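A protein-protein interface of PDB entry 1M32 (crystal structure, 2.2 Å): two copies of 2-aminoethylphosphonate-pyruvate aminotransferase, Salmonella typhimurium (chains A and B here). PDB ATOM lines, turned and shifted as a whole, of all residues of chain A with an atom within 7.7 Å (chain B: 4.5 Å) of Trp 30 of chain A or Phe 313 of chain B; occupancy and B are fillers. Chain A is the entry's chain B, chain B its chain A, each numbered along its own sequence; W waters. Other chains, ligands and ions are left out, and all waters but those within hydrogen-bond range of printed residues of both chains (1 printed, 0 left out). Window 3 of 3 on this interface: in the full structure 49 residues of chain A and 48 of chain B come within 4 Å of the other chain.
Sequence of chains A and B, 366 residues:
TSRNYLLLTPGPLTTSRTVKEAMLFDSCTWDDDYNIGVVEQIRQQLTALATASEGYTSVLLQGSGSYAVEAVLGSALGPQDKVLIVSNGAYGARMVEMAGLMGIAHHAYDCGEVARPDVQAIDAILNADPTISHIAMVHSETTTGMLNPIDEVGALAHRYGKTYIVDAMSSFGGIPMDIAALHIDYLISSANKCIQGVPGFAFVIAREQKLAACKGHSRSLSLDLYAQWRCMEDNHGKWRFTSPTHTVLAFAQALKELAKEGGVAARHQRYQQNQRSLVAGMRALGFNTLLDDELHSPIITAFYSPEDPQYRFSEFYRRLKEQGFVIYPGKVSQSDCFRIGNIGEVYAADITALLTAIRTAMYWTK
Water W1 lies within hydrogen-bond range of O of Ile 327 of chain B (2.9 Å) and SG of Cys 28 of chain A (3.3 Å).
The side-chain carboxylate of Asp 31 of chain A sits at hydrogen-bond distance from the backbone NH of Asp 33 of chain A, at 2.7 Å. The side-chain sulfur (SG) of Cys 28 of chain A lies close to the backbone NH (N) of Trp 30 of chain A, 3.7 Å away. The backbone carbonyl oxygen (O) of Thr 29 of chain A is in hydrogen-bond range of the side-chain amide nitrogen (ND2) of Asn 35 of chain A. O of Asp 31 of chain A lies within hydrogen-bond range of ND2 of Asn 35 of chain A (3.3 Å).
Trp 30 of chain A touches just these residues of chain B: Phe 313 (3.5 Å), Tyr 317 (3.7 Å) and Pro 329 (3.6 Å). Of the printed residues of chain B, Asp 31 of chain A touches Tyr 317 (2.6 Å). Phe 313 of chain B touches just one residue of chain A: Trp 30. Printed residues of chain A within 4 Å of Tyr 328 of chain B: Thr 29 (3.99 Å). The nearest residue of chain B that does not touch Trp 30 of chain A is Tyr 328 of chain B (4.3 Å). The nearest printed residue of chain A that does not touch Phe 313 of chain B is Cys 28 of chain A (8.7 Å). The nearest printed residue of chain A that does not touch Pro 329 of chain B is Cys 28 of chain A (6.5 Å).
Tyr 328 of chain B touches Thr 29 of chain A. Trp 30 of chain A touches Phe 313 of chain B (CH2 to CE1, 3.5 Å). Tyr 317 of chain B touches Trp 30 of chain A. Pro 329 of chain B touches Trp 30 of chain A.
No position is printed for both chains.
Printed residues of chain A that touch a printed residue of chain B: Thr 29, Trp 30 and Asp 31. Hydrophobic or aromatic side chains of chain A that line the printed part of chain B: Trp 30. Along chain A the printed residues that touch a printed residue of chain B span positions 29 to 31. Of the 11 printed residues of chain B, 4 touch a printed residue of chain A. Hydrophobic or aromatic side chains of chain B that line the printed part of chain A: Phe 313, Tyr 317, Tyr 328 and Pro 329. Among the printed residues, no Asp or Glu carboxylate lies within 4 Å of a Lys or Arg side-chain nitrogen of the other chain.
OH of Tyr 317 of chain B lies within hydrogen-bond range of OD2 of Asp 31 of chain A (2.6 Å).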
ATOM      1  N   SER A  27      10.170  25.519 -33.799  1.00  0.00           N
ATOM      2  CA  SER A  27      10.093  25.391 -32.352  1.00  0.00           C
ATOM      3  C   SER A  27       8.925  24.509 -31.937  1.00  0.00           C
ATOM      4  O   SER A  27       7.918  24.426 -32.641  1.00  0.00           O
ATOM      5  CB  SER A  27       9.909  26.770 -31.711  1.00  0.00           C
ATOM      6  OG  SER A  27      10.880  27.693 -32.162  1.00  0.00           O
ATOM      7  N   CYS A  28       9.066  23.837 -30.801  1.00  0.00           N
ATOM      8  CA  CYS A  28       7.975  23.019 -30.289  1.00  0.00           C
ATOM      9  C   CYS A  28       7.305  23.898 -29.245  1.00  0.00           C
ATOM     10  O   CYS A  28       7.931  24.289 -28.261  1.00  0.00           O
ATOM     11  CB  CYS A  28       8.477  21.736 -29.636  1.00  0.00           C
ATOM     12  SG  CYS A  28       7.112  20.726 -28.988  1.00  0.00           S
ATOM     13  N   THR A  29       6.037  24.213 -29.475  1.00  0.00           N
ATOM     14  CA  THR A  29       5.269  25.076 -28.585  1.00  0.00           C
ATOM     15  C   THR A  29       5.090  24.549 -27.160  1.00  0.00           C
ATOM     16  O   THR A  29       4.660  25.287 -26.273  1.00  0.00           O
ATOM     17  CB  THR A  29       3.879  25.352 -29.183  1.00  0.00           C
ATOM     18  OG1 THR A  29       3.211  24.108 -29.421  1.00  0.00           O
ATOM     19  CG2 THR A  29       4.007  26.105 -30.501  1.00  0.00           C
ATOM     20  N   TRP A  30       5.421  23.282 -26.939  1.00  0.00           N
ATOM     21  CA  TRP A  30       5.271  22.678 -25.622  1.00  0.00           C
ATOM     22  C   TRP A  30       6.592  22.571 -24.861  1.00  0.00           C
ATOM     23  O   TRP A  30       6.606  22.226 -23.677  1.00  0.00           O
ATOM     24  CB  TRP A  30       4.664  21.280 -25.769  1.00  0.00           C
ATOM     25  CG  TRP A  30       4.347  20.605 -24.465  1.00  0.00           C
ATOM     26  CD1 TRP A  30       3.233  20.791 -23.693  1.00  0.00           C
ATOM     27  CD2 TRP A  30       5.169  19.665 -23.763  1.00  0.00           C
ATOM     28  NE1 TRP A  30       3.313  20.024 -22.553  1.00  0.00           N
ATOM     29  CE2 TRP A  30       4.491  19.324 -22.570  1.00  0.00           C
ATOM     30  CE3 TRP A  30       6.415  19.079 -24.023  1.00  0.00           C
ATOM     31  CZ2 TRP A  30       5.019  18.421 -21.640  1.00  0.00           C
ATOM     32  CZ3 TRP A  30       6.940  18.181 -23.097  1.00  0.00           C
ATOM     33  CH2 TRP A  30       6.240  17.863 -21.920  1.00  0.00           C
ATOM     34  N   ASP A  31       7.701  22.880 -25.527  1.00  0.00           N
ATOM     35  CA  ASP A  31       9.014  22.762 -24.900  1.00  0.00           C
ATOM     36  C   ASP A  31       9.537  24.042 -24.242  1.00  0.00           C
ATOM     37  O   ASP A  31       9.321  25.147 -24.741  1.00  0.00           O
ATOM     38  CB  ASP A  31      10.019  22.260 -25.940  1.00  0.00           C
ATOM     39  CG  ASP A  31      11.297  21.750 -25.316  1.00  0.00           C
ATOM     40  OD1 ASP A  31      12.064  22.569 -24.774  1.00  0.00           O
ATOM     41  OD2 ASP A  31      11.527  20.524 -25.362  1.00  0.00           O
ATOM     42  N   ASP A  32      10.237  23.880 -23.123  1.00  0.00           N
ATOM     43  CA  ASP A  32      10.793  25.022 -22.401  1.00  0.00           C
ATOM     44  C   ASP A  32      11.788  25.833 -23.228  1.00  0.00           C
ATOM     45  O   ASP A  32      11.944  27.034 -23.006  1.00  0.00           O
ATOM     46  CB  ASP A  32      11.462  24.566 -21.099  1.00  0.00           C
ATOM     47  CG  ASP A  32      10.455  24.173 -20.034  1.00  0.00           C
ATOM     48  OD1 ASP A  32       9.341  24.743 -20.028  1.00  0.00           O
ATOM     49  OD2 ASP A  32      10.780  23.307 -19.193  1.00  0.00           O
ATOM     50  N   ASP A  33      12.466  25.182 -24.170  1.00  0.00           N
ATOM     51  CA  ASP A  33      13.422  25.882 -25.029  1.00  0.00           C
ATOM     52  C   ASP A  33      12.759  27.111 -25.639  1.00  0.00           C
ATOM     53  O   ASP A  33      13.386  28.154 -25.807  1.00  0.00           O
ATOM     54  CB  ASP A  33      13.896  24.988 -26.177  1.00  0.00           C
ATOM     55  CG  ASP A  33      14.783  23.855 -25.717  1.00  0.00           C
ATOM     56  OD1 ASP A  33      15.190  23.849 -24.535  1.00  0.00           O
ATOM     57  OD2 ASP A  33      15.083  22.973 -26.551  1.00  0.00           O
ATOM     58  N   TYR A  34      11.483  26.967 -25.978  1.00  0.00           N
ATOM     59  CA  TYR A  34      10.722  28.045 -26.594  1.00  0.00           C
ATOM     60  C   TYR A  34      10.061  28.943 -25.562  1.00  0.00           C
ATOM     61  O   TYR A  34      10.322  30.143 -25.513  1.00  0.00           O
ATOM     62  CB  TYR A  34       9.651  27.462 -27.521  1.00  0.00           C
ATOM     63  CG  TYR A  34       8.737  28.489 -28.148  1.00  0.00           C
ATOM     64  CD1 TYR A  34       9.235  29.455 -29.021  1.00  0.00           C
ATOM     65  CD2 TYR A  34       7.372  28.498 -27.867  1.00  0.00           C
ATOM     66  CE1 TYR A  34       8.396  30.407 -29.600  1.00  0.00           C
ATOM     67  CE2 TYR A  34       6.523  29.447 -28.440  1.00  0.00           C
ATOM     68  CZ  TYR A  34       7.042  30.398 -29.304  1.00  0.00           C
ATOM     69  OH  TYR A  34       6.209  31.350 -29.854  1.00  0.00           O
ATOM     70  N   ASN A  35       9.213  28.350 -24.730  1.00  0.00           N
ATOM     71  CA  ASN A  35       8.490  29.106 -23.720  1.00  0.00           C
ATOM     72  C   ASN A  35       9.361  29.862 -22.719  1.00  0.00           C
ATOM     73  O   ASN A  35       9.129  31.044 -22.471  1.00  0.00           O
ATOM     74  CB  ASN A  35       7.504  28.184 -23.002  1.00  0.00           C
ATOM     75  CG  ASN A  35       6.469  27.608 -23.949  1.00  0.00           C
ATOM     76  OD1 ASN A  35       5.829  28.342 -24.708  1.00  0.00           O
ATOM     77  ND2 ASN A  35       6.298  26.291 -23.915  1.00  0.00           N
ATOM     78  N   ASN A 235       2.257  28.894 -16.679  1.00  0.00           N
ATOM     79  CA  ASN A 235       3.006  27.862 -17.382  1.00  0.00           C
ATOM     80  C   ASN A 235       4.264  28.305 -18.112  1.00  0.00           C
ATOM     81  O   ASN A 235       4.520  27.882 -19.240  1.00  0.00           O
ATOM     82  CB  ASN A 235       2.080  27.124 -18.345  1.00  0.00           C
ATOM     83  CG  ASN A 235       0.773  26.728 -17.691  1.00  0.00           C
ATOM     84  OD1 ASN A 235      -0.224  27.439 -17.792  1.00  0.00           O
ATOM     85  ND2 ASN A 235       0.781  25.600 -16.995  1.00  0.00           N
ATOM     86  N   LYS A 238       3.982  29.917 -21.776  1.00  0.00           N
ATOM     87  CA  LYS A 238       3.173  29.102 -22.714  1.00  0.00           C
ATOM     88  C   LYS A 238       1.954  29.886 -23.257  1.00  0.00           C
ATOM     89  O   LYS A 238       1.194  30.499 -22.493  1.00  0.00           O
ATOM     90  CB  LYS A 238       2.640  27.851 -22.004  1.00  0.00           C
ATOM     91  CG  LYS A 238       1.580  27.102 -22.817  1.00  0.00           C
ATOM     92  CD  LYS A 238       2.186  26.157 -23.857  1.00  0.00           C
ATOM     93  CE  LYS A 238       1.199  25.098 -24.354  1.00  0.00           C
ATOM     94  NZ  LYS A 238      -0.153  25.633 -24.578  1.00  0.00           N
ATOM     95  N   THR A 245       5.695  30.973 -33.778  1.00  0.00           N
ATOM     96  CA  THR A 245       7.048  30.763 -33.275  1.00  0.00           C
ATOM     97  C   THR A 245       8.156  31.459 -34.061  1.00  0.00           C
ATOM     98  O   THR A 245       8.973  32.177 -33.489  1.00  0.00           O
ATOM     99  CB  THR A 245       7.379  29.259 -33.193  1.00  0.00           C
ATOM    100  OG1 THR A 245       7.450  28.713 -34.512  1.00  0.00           O
ATOM    101  CG2 THR A 245       6.305  28.521 -32.407  1.00  0.00           C
ATOM    102  N   TYR B 311       8.180   4.461 -15.270  1.00  0.00           N
ATOM    103  CA  TYR B 311       7.996   5.268 -16.474  1.00  0.00           C
ATOM    104  C   TYR B 311       7.509   6.684 -16.170  1.00  0.00           C
ATOM    105  O   TYR B 311       6.632   6.889 -15.333  1.00  0.00           O
ATOM    106  CB  TYR B 311       6.988   4.617 -17.429  1.00  0.00           C
ATOM    107  CG  TYR B 311       6.588   5.545 -18.559  1.00  0.00           C
ATOM    108  CD1 TYR B 311       7.435   5.758 -19.645  1.00  0.00           C
ATOM    109  CD2 TYR B 311       5.392   6.260 -18.509  1.00  0.00           C
ATOM    110  CE1 TYR B 311       7.102   6.664 -20.655  1.00  0.00           C
ATOM    111  CE2 TYR B 311       5.052   7.169 -19.509  1.00  0.00           C
ATOM    112  CZ  TYR B 311       5.911   7.365 -20.579  1.00  0.00           C
ATOM    113  OH  TYR B 311       5.579   8.262 -21.569  1.00  0.00           O
ATOM    114  N   ARG B 312       8.082   7.652 -16.873  1.00  0.00           N
ATOM    115  CA  ARG B 312       7.705   9.056 -16.731  1.00  0.00           C
ATOM    116  C   ARG B 312       7.837   9.696 -18.106  1.00  0.00           C
ATOM    117  O   ARG B 312       8.879   9.577 -18.753  1.00  0.00           O
ATOM    118  CB  ARG B 312       8.626   9.768 -15.733  1.00  0.00           C
ATOM    119  CG  ARG B 312       8.445   9.339 -14.278  1.00  0.00           C
ATOM    120  CD  ARG B 312       7.092   9.776 -13.717  1.00  0.00           C
ATOM    121  NE  ARG B 312       7.003   9.549 -12.275  1.00  0.00           N
ATOM    122  CZ  ARG B 312       6.973   8.350 -11.702  1.00  0.00           C
ATOM    123  NH1 ARG B 312       6.902   8.251 -10.380  1.00  0.00           N
ATOM    124  NH2 ARG B 312       7.001   7.249 -12.446  1.00  0.00           N
ATOM    125  N   PHE B 313       6.783  10.362 -18.569  1.00  0.00           N
ATOM    126  CA  PHE B 313       6.844  10.993 -19.881  1.00  0.00           C
ATOM    127  C   PHE B 313       7.943  12.041 -19.932  1.00  0.00           C
ATOM    128  O   PHE B 313       8.624  12.184 -20.946  1.00  0.00           O
ATOM    129  CB  PHE B 313       5.506  11.637 -20.248  1.00  0.00           C
ATOM    130  CG  PHE B 313       5.545  12.409 -21.542  1.00  0.00           C
ATOM    131  CD1 PHE B 313       5.673  13.795 -21.538  1.00  0.00           C
ATOM    132  CD2 PHE B 313       5.490  11.746 -22.765  1.00  0.00           C
ATOM    133  CE1 PHE B 313       5.746  14.510 -22.737  1.00  0.00           C
ATOM    134  CE2 PHE B 313       5.564  12.449 -23.968  1.00  0.00           C
ATOM    135  CZ  PHE B 313       5.691  13.833 -23.957  1.00  0.00           C
ATOM    136  N   SER B 314       8.121  12.767 -18.833  1.00  0.00           N
ATOM    137  CA  SER B 314       9.145  13.802 -18.779  1.00  0.00           C
ATOM    138  C   SER B 314      10.515  13.221 -19.117  1.00  0.00           C
ATOM    139  O   SER B 314      11.272  13.809 -19.882  1.00  0.00           O
ATOM    140  CB  SER B 314       9.184  14.443 -17.386  1.00  0.00           C
ATOM    141  OG  SER B 314       9.529  13.491 -16.392  1.00  0.00           O
ATOM    142  N   GLU B 315      10.819  12.056 -18.552  1.00  0.00           N
ATOM    143  CA  GLU B 315      12.103  11.408 -18.787  1.00  0.00           C
ATOM    144  C   GLU B 315      12.175  10.767 -20.180  1.00  0.00           C
ATOM    145  O   GLU B 315      13.183  10.886 -20.878  1.00  0.00           O
ATOM    146  CB  GLU B 315      12.360  10.362 -17.700  1.00  0.00           C
ATOM    147  CG  GLU B 315      13.799   9.877 -17.650  1.00  0.00           C
ATOM    148  CD  GLU B 315      14.784  11.013 -17.443  1.00  0.00           C
ATOM    149  OE1 GLU B 315      15.892  10.935 -18.009  1.00  0.00           O
ATOM    150  OE2 GLU B 315      14.457  11.978 -16.713  1.00  0.00           O
ATOM    151  N   PHE B 316      11.102  10.093 -20.580  1.00  0.00           N
ATOM    152  CA  PHE B 316      11.040   9.452 -21.891  1.00  0.00           C
ATOM    153  C   PHE B 316      11.262  10.535 -22.954  1.00  0.00           C
ATOM    154  O   PHE B 316      12.074  10.386 -23.863  1.00  0.00           O
ATOM    155  CB  PHE B 316       9.661   8.810 -22.079  1.00  0.00           C
ATOM    156  CG  PHE B 316       9.523   7.991 -23.337  1.00  0.00           C
ATOM    157  CD1 PHE B 316       8.291   7.905 -23.986  1.00  0.00           C
ATOM    158  CD2 PHE B 316      10.603   7.278 -23.852  1.00  0.00           C
ATOM    159  CE1 PHE B 316       8.131   7.122 -25.129  1.00  0.00           C
ATOM    160  CE2 PHE B 316      10.458   6.490 -24.995  1.00  0.00           C
ATOM    161  CZ  PHE B 316       9.217   6.412 -25.635  1.00  0.00           C
ATOM    162  N   TYR B 317      10.534  11.635 -22.810  1.00  0.00           N
ATOM    163  CA  TYR B 317      10.618  12.759 -23.731  1.00  0.00           C
ATOM    164  C   TYR B 317      12.022  13.356 -23.831  1.00  0.00           C
ATOM    165  O   TYR B 317      12.524  13.594 -24.930  1.00  0.00           O
ATOM    166  CB  TYR B 317       9.607  13.829 -23.297  1.00  0.00           C
ATOM    167  CG  TYR B 317       9.661  15.124 -24.069  1.00  0.00           C
ATOM    168  CD1 TYR B 317      10.535  16.147 -23.695  1.00  0.00           C
ATOM    169  CD2 TYR B 317       8.816  15.343 -25.155  1.00  0.00           C
ATOM    170  CE1 TYR B 317      10.562  17.358 -24.382  1.00  0.00           C
ATOM    171  CE2 TYR B 317       8.836  16.552 -25.853  1.00  0.00           C
ATOM    172  CZ  TYR B 317       9.709  17.554 -25.460  1.00  0.00           C
ATOM    173  OH  TYR B 317       9.725  18.753 -26.139  1.00  0.00           O
ATOM    174  N   ILE B 327       8.677  14.122 -29.278  1.00  0.00           N
ATOM    175  CA  ILE B 327       7.335  13.576 -29.371  1.00  0.00           C
ATOM    176  C   ILE B 327       6.360  14.541 -28.708  1.00  0.00           C
ATOM    177  O   ILE B 327       6.706  15.687 -28.437  1.00  0.00           O
ATOM    178  CB  ILE B 327       7.219  12.157 -28.748  1.00  0.00           C
ATOM    179  CG1 ILE B 327       7.676  12.159 -27.293  1.00  0.00           C
ATOM    180  CG2 ILE B 327       8.028  11.170 -29.577  1.00  0.00           C
ATOM    181  CD1 ILE B 327       7.506  10.806 -26.612  1.00  0.00           C
ATOM    182  N   TYR B 328       5.150  14.079 -28.428  1.00  0.00           N
ATOM    183  CA  TYR B 328       4.142  14.964 -27.871  1.00  0.00           C
ATOM    184  C   TYR B 328       3.389  14.381 -26.679  1.00  0.00           C
ATOM    185  O   TYR B 328       3.137  13.181 -26.611  1.00  0.00           O
ATOM    186  CB  TYR B 328       3.149  15.302 -28.983  1.00  0.00           C
ATOM    187  CG  TYR B 328       2.654  16.727 -29.008  1.00  0.00           C
ATOM    188  CD1 TYR B 328       1.289  17.001 -29.027  1.00  0.00           C
ATOM    189  CD2 TYR B 328       3.545  17.800 -29.083  1.00  0.00           C
ATOM    190  CE1 TYR B 328       0.820  18.303 -29.128  1.00  0.00           C
ATOM    191  CE2 TYR B 328       3.085  19.108 -29.184  1.00  0.00           C
ATOM    192  CZ  TYR B 328       1.720  19.352 -29.209  1.00  0.00           C
ATOM    193  OH  TYR B 328       1.248  20.640 -29.337  1.00  0.00           O
ATOM    194  N   PRO B 329       3.021  15.234 -25.714  1.00  0.00           N
ATOM    195  CA  PRO B 329       2.287  14.729 -24.553  1.00  0.00           C
ATOM    196  C   PRO B 329       0.859  14.382 -24.953  1.00  0.00           C
ATOM    197  O   PRO B 329       0.329  14.919 -25.924  1.00  0.00           O
ATOM    198  CB  PRO B 329       2.348  15.898 -23.573  1.00  0.00           C
ATOM    199  CG  PRO B 329       2.357  17.091 -24.487  1.00  0.00           C
ATOM    200  CD  PRO B 329       3.328  16.666 -25.565  1.00  0.00           C
ATOM    201  N   PHE B 338       0.494   9.230 -24.568  1.00  0.00           N
ATOM    202  CA  PHE B 338       1.468  10.144 -25.135  1.00  0.00           C
ATOM    203  C   PHE B 338       1.213  10.045 -26.636  1.00  0.00           C
ATOM    204  O   PHE B 338       0.610   9.076 -27.097  1.00  0.00           O
ATOM    205  CB  PHE B 338       2.908   9.755 -24.748  1.00  0.00           C
ATOM    206  CG  PHE B 338       3.402   8.472 -25.361  1.00  0.00           C
ATOM    207  CD1 PHE B 338       4.002   8.470 -26.619  1.00  0.00           C
ATOM    208  CD2 PHE B 338       3.319   7.274 -24.656  1.00  0.00           C
ATOM    209  CE1 PHE B 338       4.517   7.296 -27.163  1.00  0.00           C
ATOM    210  CE2 PHE B 338       3.830   6.096 -25.190  1.00  0.00           C
ATOM    211  CZ  PHE B 338       4.432   6.108 -26.445  1.00  0.00           C
HETATM  212  O   HOH W   1       6.252  18.198 -27.122  1.00  0.00           O
